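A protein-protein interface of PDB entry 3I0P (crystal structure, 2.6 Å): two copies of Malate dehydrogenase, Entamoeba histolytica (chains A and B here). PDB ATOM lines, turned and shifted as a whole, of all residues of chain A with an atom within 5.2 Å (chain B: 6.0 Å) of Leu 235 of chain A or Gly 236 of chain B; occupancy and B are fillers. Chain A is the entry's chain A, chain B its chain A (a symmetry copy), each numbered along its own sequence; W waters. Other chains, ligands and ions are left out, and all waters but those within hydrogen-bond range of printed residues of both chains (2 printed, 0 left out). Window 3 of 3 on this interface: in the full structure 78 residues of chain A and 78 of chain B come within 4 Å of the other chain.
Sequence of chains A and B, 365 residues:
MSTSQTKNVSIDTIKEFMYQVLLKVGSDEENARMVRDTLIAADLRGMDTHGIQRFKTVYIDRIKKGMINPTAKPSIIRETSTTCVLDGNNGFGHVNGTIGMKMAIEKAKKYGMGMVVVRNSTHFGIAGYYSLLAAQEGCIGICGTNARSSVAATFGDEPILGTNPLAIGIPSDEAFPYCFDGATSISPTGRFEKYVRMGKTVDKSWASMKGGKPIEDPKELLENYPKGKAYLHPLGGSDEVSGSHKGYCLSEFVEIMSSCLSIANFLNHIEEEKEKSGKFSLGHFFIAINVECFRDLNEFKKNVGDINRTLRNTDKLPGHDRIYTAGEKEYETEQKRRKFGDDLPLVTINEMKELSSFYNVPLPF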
ATOM      1  N   THR A 184     -23.256 -21.787 -27.378  1.00  0.00           N
ATOM      2  CA  THR A 184     -22.337 -22.804 -27.886  1.00  0.00           C
ATOM      3  C   THR A 184     -20.923 -22.241 -28.073  1.00  0.00           C
ATOM      4  O   THR A 184     -19.975 -22.989 -28.306  1.00  0.00           O
ATOM      5  CB  THR A 184     -22.850 -23.431 -29.177  1.00  0.00           C
ATOM      6  OG1 THR A 184     -23.364 -22.400 -30.030  1.00  0.00           O
ATOM      7  CG2 THR A 184     -23.961 -24.444 -28.877  1.00  0.00           C
ATOM      8  N   SER A 185     -20.790 -20.918 -27.985  1.00  0.00           N
ATOM      9  CA  SER A 185     -19.490 -20.275 -27.790  1.00  0.00           C
ATOM     10  C   SER A 185     -19.176 -20.245 -26.288  1.00  0.00           C
ATOM     11  O   SER A 185     -20.097 -20.285 -25.457  1.00  0.00           O
ATOM     12  CB  SER A 185     -19.505 -18.854 -28.358  1.00  0.00           C
ATOM     13  OG  SER A 185     -20.505 -18.072 -27.735  1.00  0.00           O
ATOM     14  N   ILE A 186     -17.893 -20.187 -25.930  1.00  0.00           N
ATOM     15  CA  ILE A 186     -17.513 -20.130 -24.514  1.00  0.00           C
ATOM     16  C   ILE A 186     -18.262 -18.990 -23.809  1.00  0.00           C
ATOM     17  O   ILE A 186     -18.870 -19.193 -22.759  1.00  0.00           O
ATOM     18  CB  ILE A 186     -15.971 -19.990 -24.301  1.00  0.00           C
ATOM     19  CG1 ILE A 186     -15.226 -21.164 -24.961  1.00  0.00           C
ATOM     20  CG2 ILE A 186     -15.645 -19.888 -22.802  1.00  0.00           C
ATOM     21  CD1 ILE A 186     -13.703 -21.113 -24.858  1.00  0.00           C
ATOM     22  N   HIS A 233     -14.766 -17.284 -29.725  1.00  0.00           N
ATOM     23  CA  HIS A 233     -14.426 -18.693 -29.985  1.00  0.00           C
ATOM     24  C   HIS A 233     -15.563 -19.622 -29.587  1.00  0.00           C
ATOM     25  O   HIS A 233     -16.310 -19.322 -28.651  1.00  0.00           O
ATOM     26  CB  HIS A 233     -13.152 -19.103 -29.241  1.00  0.00           C
ATOM     27  CG  HIS A 233     -11.938 -18.341 -29.669  1.00  0.00           C
ATOM     28  ND1 HIS A 233     -11.380 -18.473 -30.924  1.00  0.00           N
ATOM     29  CD2 HIS A 233     -11.185 -17.424 -29.016  1.00  0.00           C
ATOM     30  CE1 HIS A 233     -10.332 -17.676 -31.021  1.00  0.00           C
ATOM     31  NE2 HIS A 233     -10.192 -17.030 -29.877  1.00  0.00           N
ATOM     32  N   PRO A 234     -15.696 -20.761 -30.288  1.00  0.00           N
ATOM     33  CA  PRO A 234     -16.664 -21.768 -29.857  1.00  0.00           C
ATOM     34  C   PRO A 234     -16.229 -22.422 -28.547  1.00  0.00           C
ATOM     35  O   PRO A 234     -15.061 -22.314 -28.160  1.00  0.00           O
ATOM     36  CB  PRO A 234     -16.614 -22.809 -30.985  1.00  0.00           C
ATOM     37  CG  PRO A 234     -15.849 -22.169 -32.108  1.00  0.00           C
ATOM     38  CD  PRO A 234     -14.933 -21.199 -31.466  1.00  0.00           C
ATOM     39  N   LEU A 235     -17.158 -23.087 -27.865  1.00  0.00           N
ATOM     40  CA  LEU A 235     -16.776 -23.987 -26.774  1.00  0.00           C
ATOM     41  C   LEU A 235     -15.692 -24.976 -27.272  1.00  0.00           C
ATOM     42  O   LEU A 235     -15.867 -25.668 -28.281  1.00  0.00           O
ATOM     43  CB  LEU A 235     -18.000 -24.707 -26.200  1.00  0.00           C
ATOM     44  CG  LEU A 235     -17.815 -25.805 -25.148  1.00  0.00           C
ATOM     45  CD1 LEU A 235     -17.230 -25.269 -23.843  1.00  0.00           C
ATOM     46  CD2 LEU A 235     -19.130 -26.532 -24.893  1.00  0.00           C
ATOM     47  N   GLY A 236     -14.558 -24.993 -26.581  1.00  0.00           N
ATOM     48  CA  GLY A 236     -13.408 -25.769 -27.027  1.00  0.00           C
ATOM     49  C   GLY A 236     -12.279 -24.897 -27.553  1.00  0.00           C
ATOM     50  O   GLY A 236     -11.207 -25.401 -27.890  1.00  0.00           O
ATOM     51  N   GLY A 237     -12.520 -23.590 -27.633  1.00  0.00           N
ATOM     52  CA  GLY A 237     -11.487 -22.639 -28.033  1.00  0.00           C
ATOM     53  C   GLY A 237     -11.228 -22.618 -29.523  1.00  0.00           C
ATOM     54  O   GLY A 237     -12.149 -22.742 -30.332  1.00  0.00           O
ATOM     55  N   SER A 242      -8.042 -28.707 -27.831  1.00  0.00           N
ATOM     56  CA  SER A 242      -8.840 -28.402 -26.650  1.00  0.00           C
ATOM     57  C   SER A 242     -10.327 -28.697 -26.882  1.00  0.00           C
ATOM     58  O   SER A 242     -11.127 -28.601 -25.952  1.00  0.00           O
ATOM     59  CB  SER A 242      -8.622 -26.951 -26.210  1.00  0.00           C
ATOM     60  OG  SER A 242      -8.805 -26.071 -27.301  1.00  0.00           O
ATOM     61  N   GLY A 243     -10.682 -29.053 -28.120  1.00  0.00           N
ATOM     62  CA  GLY A 243     -12.050 -29.450 -28.463  1.00  0.00           C
ATOM     63  C   GLY A 243     -12.856 -28.457 -29.287  1.00  0.00           C
ATOM     64  O   GLY A 243     -14.080 -28.592 -29.404  1.00  0.00           O
ATOM     65  N   SER A 244     -12.173 -27.470 -29.868  1.00  0.00           N
ATOM     66  CA  SER A 244     -12.801 -26.403 -30.664  1.00  0.00           C
ATOM     67  C   SER A 244     -13.852 -26.880 -31.642  1.00  0.00           C
ATOM     68  O   SER A 244     -14.931 -26.307 -31.727  1.00  0.00           O
ATOM     69  CB  SER A 244     -11.738 -25.641 -31.454  1.00  0.00           C
ATOM     70  OG  SER A 244     -12.341 -24.728 -32.353  1.00  0.00           O
ATOM     71  N   LYS A 246     -15.765 -29.314 -31.659  1.00  0.00           N
ATOM     72  CA  LYS A 246     -17.008 -29.759 -31.047  1.00  0.00           C
ATOM     73  C   LYS A 246     -17.987 -28.596 -30.815  1.00  0.00           C
ATOM     74  O   LYS A 246     -19.100 -28.617 -31.344  1.00  0.00           O
ATOM     75  CB  LYS A 246     -16.733 -30.590 -29.783  1.00  0.00           C
ATOM     76  CG  LYS A 246     -15.928 -31.855 -30.085  1.00  0.00           C
ATOM     77  CD  LYS A 246     -15.595 -32.647 -28.853  1.00  0.00           C
ATOM     78  CE  LYS A 246     -14.983 -33.986 -29.241  1.00  0.00           C
ATOM     79  NZ  LYS A 246     -14.991 -34.958 -28.114  1.00  0.00           N
ATOM     80  N   GLY A 247     -17.577 -27.576 -30.063  1.00  0.00           N
ATOM     81  CA  GLY A 247     -18.424 -26.399 -29.853  1.00  0.00           C
ATOM     82  C   GLY A 247     -18.865 -25.804 -31.182  1.00  0.00           C
ATOM     83  O   GLY A 247     -20.038 -25.450 -31.364  1.00  0.00           O
ATOM     84  N   TYR A 248     -17.922 -25.719 -32.118  1.00  0.00           N
ATOM     85  CA  TYR A 248     -18.195 -25.242 -33.471  1.00  0.00           C
ATOM     86  C   TYR A 248     -19.287 -26.073 -34.169  1.00  0.00           C
ATOM     87  O   TYR A 248     -20.255 -25.509 -34.686  1.00  0.00           O
ATOM     88  CB  TYR A 248     -16.884 -25.195 -34.266  1.00  0.00           C
ATOM     89  CG  TYR A 248     -16.998 -25.141 -35.769  1.00  0.00           C
ATOM     90  CD1 TYR A 248     -17.900 -24.272 -36.406  1.00  0.00           C
ATOM     91  CD2 TYR A 248     -16.175 -25.942 -36.569  1.00  0.00           C
ATOM     92  CE1 TYR A 248     -17.997 -24.228 -37.799  1.00  0.00           C
ATOM     93  CE2 TYR A 248     -16.249 -25.890 -37.965  1.00  0.00           C
ATOM     94  CZ  TYR A 248     -17.160 -25.032 -38.569  1.00  0.00           C
ATOM     95  OH  TYR A 248     -17.240 -24.997 -39.941  1.00  0.00           O
ATOM     96  N   LEU A 250     -21.497 -27.979 -32.699  1.00  0.00           N
ATOM     97  CA  LEU A 250     -22.721 -27.811 -31.910  1.00  0.00           C
ATOM     98  C   LEU A 250     -23.424 -26.485 -32.232  1.00  0.00           C
ATOM     99  O   LEU A 250     -24.644 -26.445 -32.385  1.00  0.00           O
ATOM    100  CB  LEU A 250     -22.442 -27.956 -30.405  1.00  0.00           C
ATOM    101  CG  LEU A 250     -22.021 -29.354 -29.898  1.00  0.00           C
ATOM    102  CD1 LEU A 250     -21.546 -29.315 -28.432  1.00  0.00           C
ATOM    103  CD2 LEU A 250     -23.109 -30.418 -30.088  1.00  0.00           C
ATOM    104  N   ILE B 186     -13.401 -33.840 -23.752  1.00  0.00           N
ATOM    105  CA  ILE B 186     -12.487 -33.416 -24.818  1.00  0.00           C
ATOM    106  C   ILE B 186     -11.959 -34.638 -25.583  1.00  0.00           C
ATOM    107  O   ILE B 186     -12.012 -34.681 -26.811  1.00  0.00           O
ATOM    108  CB  ILE B 186     -11.302 -32.540 -24.294  1.00  0.00           C
ATOM    109  CG1 ILE B 186     -11.832 -31.287 -23.577  1.00  0.00           C
ATOM    110  CG2 ILE B 186     -10.359 -32.170 -25.452  1.00  0.00           C
ATOM    111  CD1 ILE B 186     -10.764 -30.374 -22.980  1.00  0.00           C
ATOM    112  N   PRO B 234     -14.265 -32.770 -19.034  1.00  0.00           N
ATOM    113  CA  PRO B 234     -15.322 -32.516 -20.011  1.00  0.00           C
ATOM    114  C   PRO B 234     -14.856 -31.527 -21.078  1.00  0.00           C
ATOM    115  O   PRO B 234     -13.857 -30.828 -20.880  1.00  0.00           O
ATOM    116  CB  PRO B 234     -16.432 -31.870 -19.169  1.00  0.00           C
ATOM    117  CG  PRO B 234     -16.041 -32.080 -17.735  1.00  0.00           C
ATOM    118  CD  PRO B 234     -14.563 -32.159 -17.730  1.00  0.00           C
ATOM    119  N   LEU B 235     -15.567 -31.472 -22.202  1.00  0.00           N
ATOM    120  CA  LEU B 235     -15.384 -30.362 -23.141  1.00  0.00           C
ATOM    121  C   LEU B 235     -15.508 -29.016 -22.385  1.00  0.00           C
ATOM    122  O   LEU B 235     -16.497 -28.757 -21.689  1.00  0.00           O
ATOM    123  CB  LEU B 235     -16.368 -30.464 -24.311  1.00  0.00           C
ATOM    124  CG  LEU B 235     -16.453 -29.328 -25.337  1.00  0.00           C
ATOM    125  CD1 LEU B 235     -15.161 -29.167 -26.135  1.00  0.00           C
ATOM    126  CD2 LEU B 235     -17.642 -29.533 -26.268  1.00  0.00           C
ATOM    127  N   GLY B 236     -14.472 -28.192 -22.490  1.00  0.00           N
ATOM    128  CA  GLY B 236     -14.399 -26.961 -21.713  1.00  0.00           C
ATOM    129  C   GLY B 236     -13.363 -27.027 -20.603  1.00  0.00           C
ATOM    130  O   GLY B 236     -13.125 -26.035 -19.912  1.00  0.00           O
ATOM    131  N   GLY B 237     -12.752 -28.196 -20.423  1.00  0.00           N
ATOM    132  CA  GLY B 237     -11.674 -28.361 -19.453  1.00  0.00           C
ATOM    133  C   GLY B 237     -12.156 -28.465 -18.023  1.00  0.00           C
ATOM    134  O   GLY B 237     -13.192 -29.070 -17.742  1.00  0.00           O
ATOM    135  N   SER B 238     -11.398 -27.880 -17.105  1.00  0.00           N
ATOM    136  CA  SER B 238     -11.702 -28.003 -15.677  1.00  0.00           C
ATOM    137  C   SER B 238     -12.162 -26.697 -15.054  1.00  0.00           C
ATOM    138  O   SER B 238     -12.781 -26.714 -13.997  1.00  0.00           O
ATOM    139  CB  SER B 238     -10.511 -28.581 -14.901  1.00  0.00           C
ATOM    140  OG  SER B 238      -9.283 -28.080 -15.395  1.00  0.00           O
ATOM    141  N   ASP B 239     -11.859 -25.581 -15.712  1.00  0.00           N
ATOM    142  CA  ASP B 239     -12.289 -24.261 -15.249  1.00  0.00           C
ATOM    143  C   ASP B 239     -13.532 -23.781 -15.995  1.00  0.00           C
ATOM    144  O   ASP B 239     -13.637 -23.926 -17.224  1.00  0.00           O
ATOM    145  CB  ASP B 239     -11.177 -23.209 -15.419  1.00  0.00           C
ATOM    146  CG  ASP B 239      -9.825 -23.669 -14.895  1.00  0.00           C
ATOM    147  OD1 ASP B 239      -9.740 -24.181 -13.750  1.00  0.00           O
ATOM    148  OD2 ASP B 239      -8.839 -23.502 -15.636  1.00  0.00           O
ATOM    149  N   GLU B 240     -14.454 -23.187 -15.235  1.00  0.00           N
ATOM    150  CA  GLU B 240     -15.656 -22.558 -15.781  1.00  0.00           C
ATOM    151  C   GLU B 240     -15.288 -21.493 -16.803  1.00  0.00           C
ATOM    152  O   GLU B 240     -16.046 -21.226 -17.748  1.00  0.00           O
ATOM    153  CB  GLU B 240     -16.459 -21.901 -14.667  1.00  0.00           C
ATOM    154  CG  GLU B 240     -17.111 -22.867 -13.722  1.00  0.00           C
ATOM    155  CD  GLU B 240     -17.888 -22.160 -12.640  1.00  0.00           C
ATOM    156  OE1 GLU B 240     -17.577 -20.982 -12.356  1.00  0.00           O
ATOM    157  OE2 GLU B 240     -18.804 -22.783 -12.070  1.00  0.00           O
ATOM    158  N   VAL B 241     -14.111 -20.904 -16.600  1.00  0.00           N
ATOM    159  CA  VAL B 241     -13.634 -19.822 -17.442  1.00  0.00           C
ATOM    160  C   VAL B 241     -13.464 -20.275 -18.904  1.00  0.00           C
ATOM    161  O   VAL B 241     -13.720 -19.506 -19.829  1.00  0.00           O
ATOM    162  CB  VAL B 241     -12.362 -19.126 -16.827  1.00  0.00           C
ATOM    163  CG1 VAL B 241     -11.072 -19.894 -17.114  1.00  0.00           C
ATOM    164  CG2 VAL B 241     -12.257 -17.699 -17.308  1.00  0.00           C
ATOM    165  N   SER B 242     -13.069 -21.530 -19.101  1.00  0.00           N
ATOM    166  CA  SER B 242     -12.875 -22.060 -20.445  1.00  0.00           C
ATOM    167  C   SER B 242     -14.128 -22.785 -20.953  1.00  0.00           C
ATOM    168  O   SER B 242     -14.174 -23.196 -22.112  1.00  0.00           O
ATOM    169  CB  SER B 242     -11.646 -22.973 -20.496  1.00  0.00           C
ATOM    170  OG  SER B 242     -11.710 -23.945 -19.472  1.00  0.00           O
ATOM    171  N   GLY B 243     -15.129 -22.933 -20.082  1.00  0.00           N
ATOM    172  CA  GLY B 243     -16.417 -23.525 -20.456  1.00  0.00           C
ATOM    173  C   GLY B 243     -16.698 -24.923 -19.926  1.00  0.00           C
ATOM    174  O   GLY B 243     -17.630 -25.590 -20.390  1.00  0.00           O
ATOM    175  N   SER B 244     -15.907 -25.361 -18.946  1.00  0.00           N
ATOM    176  CA  SER B 244     -16.014 -26.702 -18.349  1.00  0.00           C
ATOM    177  C   SER B 244     -17.427 -27.142 -18.035  1.00  0.00           C
ATOM    178  O   SER B 244     -17.816 -28.260 -18.347  1.00  0.00           O
ATOM    179  CB  SER B 244     -15.206 -26.768 -17.054  1.00  0.00           C
ATOM    180  OG  SER B 244     -15.439 -27.991 -16.380  1.00  0.00           O
ATOM    181  N   HIS B 245     -18.173 -26.256 -17.388  1.00  0.00           N
ATOM    182  CA  HIS B 245     -19.540 -26.532 -16.941  1.00  0.00           C
ATOM    183  C   HIS B 245     -20.466 -26.940 -18.078  1.00  0.00           C
ATOM    184  O   HIS B 245     -21.414 -27.706 -17.876  1.00  0.00           O
ATOM    185  CB  HIS B 245     -20.113 -25.330 -16.178  1.00  0.00           C
ATOM    186  CG  HIS B 245     -20.041 -24.035 -16.925  1.00  0.00           C
ATOM    187  ND1 HIS B 245     -18.848 -23.428 -17.255  1.00  0.00           N
ATOM    188  CD2 HIS B 245     -21.017 -23.219 -17.386  1.00  0.00           C
ATOM    189  CE1 HIS B 245     -19.090 -22.307 -17.910  1.00  0.00           C
ATOM    190  NE2 HIS B 245     -20.400 -22.153 -17.998  1.00  0.00           N
ATOM    191  N   LYS B 246     -20.176 -26.443 -19.277  1.00  0.00           N
ATOM    192  CA  LYS B 246     -20.987 -26.762 -20.443  1.00  0.00           C
ATOM    193  C   LYS B 246     -20.806 -28.222 -20.891  1.00  0.00           C
ATOM    194  O   LYS B 246     -21.778 -28.977 -20.925  1.00  0.00           O
ATOM    195  CB  LYS B 246     -20.754 -25.742 -21.570  1.00  0.00           C
ATOM    196  CG  LYS B 246     -21.142 -24.322 -21.156  1.00  0.00           C
ATOM    197  CD  LYS B 246     -20.863 -23.302 -22.222  1.00  0.00           C
ATOM    198  CE  LYS B 246     -21.460 -21.957 -21.831  1.00  0.00           C
ATOM    199  NZ  LYS B 246     -21.559 -21.025 -22.987  1.00  0.00           N
ATOM    200  N   GLY B 247     -19.577 -28.632 -21.201  1.00  0.00           N
ATOM    201  CA  GLY B 247     -19.311 -30.025 -21.567  1.00  0.00           C
ATOM    202  C   GLY B 247     -19.825 -30.975 -20.497  1.00  0.00           C
ATOM    203  O   GLY B 247     -20.452 -32.000 -20.800  1.00  0.00           O
ATOM    204  N   LEU B 250     -23.551 -31.167 -20.696  1.00  0.00           N
ATOM    205  CA  LEU B 250     -23.893 -31.918 -21.908  1.00  0.00           C
ATOM    206  C   LEU B 250     -23.679 -33.425 -21.717  1.00  0.00           C
ATOM    207  O   LEU B 250     -24.517 -34.231 -22.120  1.00  0.00           O
ATOM    208  CB  LEU B 250     -23.130 -31.385 -23.131  1.00  0.00           C
ATOM    209  CG  LEU B 250     -23.488 -29.964 -23.621  1.00  0.00           C
ATOM    210  CD1 LEU B 250     -22.502 -29.459 -24.693  1.00  0.00           C
ATOM    211  CD2 LEU B 250     -24.935 -29.842 -24.115  1.00  0.00           C
HETATM  212  O   HOH W   1     -11.960 -27.237 -23.735  1.00  0.00           O
HETATM  213  O   HOH W   2     -12.891 -24.392 -24.207  1.00  0.00           O
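Ile 186 of chain A touches Lys 246 of chain B, and with the chains exchanged Lys 246 of chain A touches Ile 186 of chain B.
Leu 235 of chain B touches its own counterpart, Leu 235 of chain A.
Leu 235 of chain A touches Lys 246 of chain B, and with the chains exchanged Lys 246 of chain A touches Leu 235 of chain B.
Leu 250 of chain B touches its own counterpart, Leu 250 of chain A.
Positions printed for both chains: 186, 234, 235, 236, 237, 242, 243, 244, 246, 247 and 250.
Of the 14 pairs that touch across the chains among the printed residues, 12 have their exchanged pair printed and touching as well.
The backbone NH (N) of Ile 186 of chain A sits at hydrogen-bond distance from the backbone carbonyl oxygen (O) of His 233 of chain A, 3.3 Å away.
O of Leu 235 of chain A lies close to N of Gly 247 of chain A, 3.1 Å away.
The backbone carbonyl oxygen of Gly 236 of chain A is in hydrogen-bond range of the side-chain hydroxyl of Ser 242 of chain A.
O of Gly 236 of chain A sits at hydrogen-bond distance from N of Ser 244 of chain A, 3.0 Å away.
O of Leu 235 of chain B sits close to N of Gly 247 of chain B (3.1 Å).
The backbone carbonyl oxygen of Gly 236 of chain B lies within hydrogen-bond range of the backbone NH of Ser 244 of chain B.
Water W1 lies within hydrogen-bond range of the backbone carbonyl oxygen (O) of Ser 242 of chain A (2.7 Å) and the backbone NH (N) of Gly 236 of chain B (3.0 Å).
Water W2 lies within hydrogen-bond range of O of Ser 242 of chain B and N of Gly 236 of chain A.
NZ of Lys 246 of chain B is in hydrogen-bond range of O of Ser 185 of chain A, at 3.0 Å.
The backbone carbonyl oxygen (O) of Ile 186 of chain A sits at hydrogen-bond distance from the side-chain amino group (NZ) of Lys 246 of chain B.
The side-chain amino group (NZ) of Lys 246 of chain A sits at hydrogen-bond distance from the backbone carbonyl oxygen (O) of Ile 186 of chain B (3.3 Å).
Leu 235 of chain A touches four residues of chain B.
Of chain A, only Leu 235 comes within 4 Å of Gly 236 of chain B.
Of the printed residues of chain A, Ile 186 of chain B touches Ser 242 (3.5 Å) and Lys 246 (3.3 Å).
Of the printed residues of chain B, Leu 250 of chain A touches Leu 250.
Of the printed residues of chain B, Gly 243 of chain A touches Leu 235 (3.5 Å).
The nearest residue of chain B that does not touch Leu 235 of chain A is Ser 242 of chain B (4.1 Å).
Among the printed residues, pairs that only touch across the chains: Ile 186 of chain A with Ser 242 of chain B (3.5 Å), Ser 242 of chain A with Ile 186 of chain B (3.5 Å), Gly 243 of chain A with Leu 235 of chain B (3.5 Å), Leu 235 of chain A with Gly 243 of chain B (3.5 Å), Ile 186 of chain A with Val 241 of chain B (3.6 Å), Leu 235 of chain A with Leu 235 of chain B (3.6 Å), Lys 246 of chain A with Leu 235 of chain B (3.8 Å), Leu 235 of chain A with Lys 246 of chain B (3.8 Å), Leu 250 of chain A with Leu 250 of chain B (3.9 Å), Leu 235 of chain A with Gly 236 of chain B (3.9 Å) and Gly 236 of chain A with Leu 235 of chain B (3.9 Å).
Hydrophobic or aromatic side chains of chain A within 4 Å of the printed part of chain B: Ile 186, Leu 235 and Leu 250.
Printed residues of chain B that touch a printed residue of chain A: Ile 186, Leu 235, Gly 236, Val 241, Ser 242, Gly 243, Lys 246 and Leu 250.
Along chain B the printed residues that touch a printed residue of chain A span positions 186 to 250.
Among the printed residues, no Asp or Glu carboxylate lies within 4 Å of a Lys or Arg side-chain nitrogen of the other chain.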
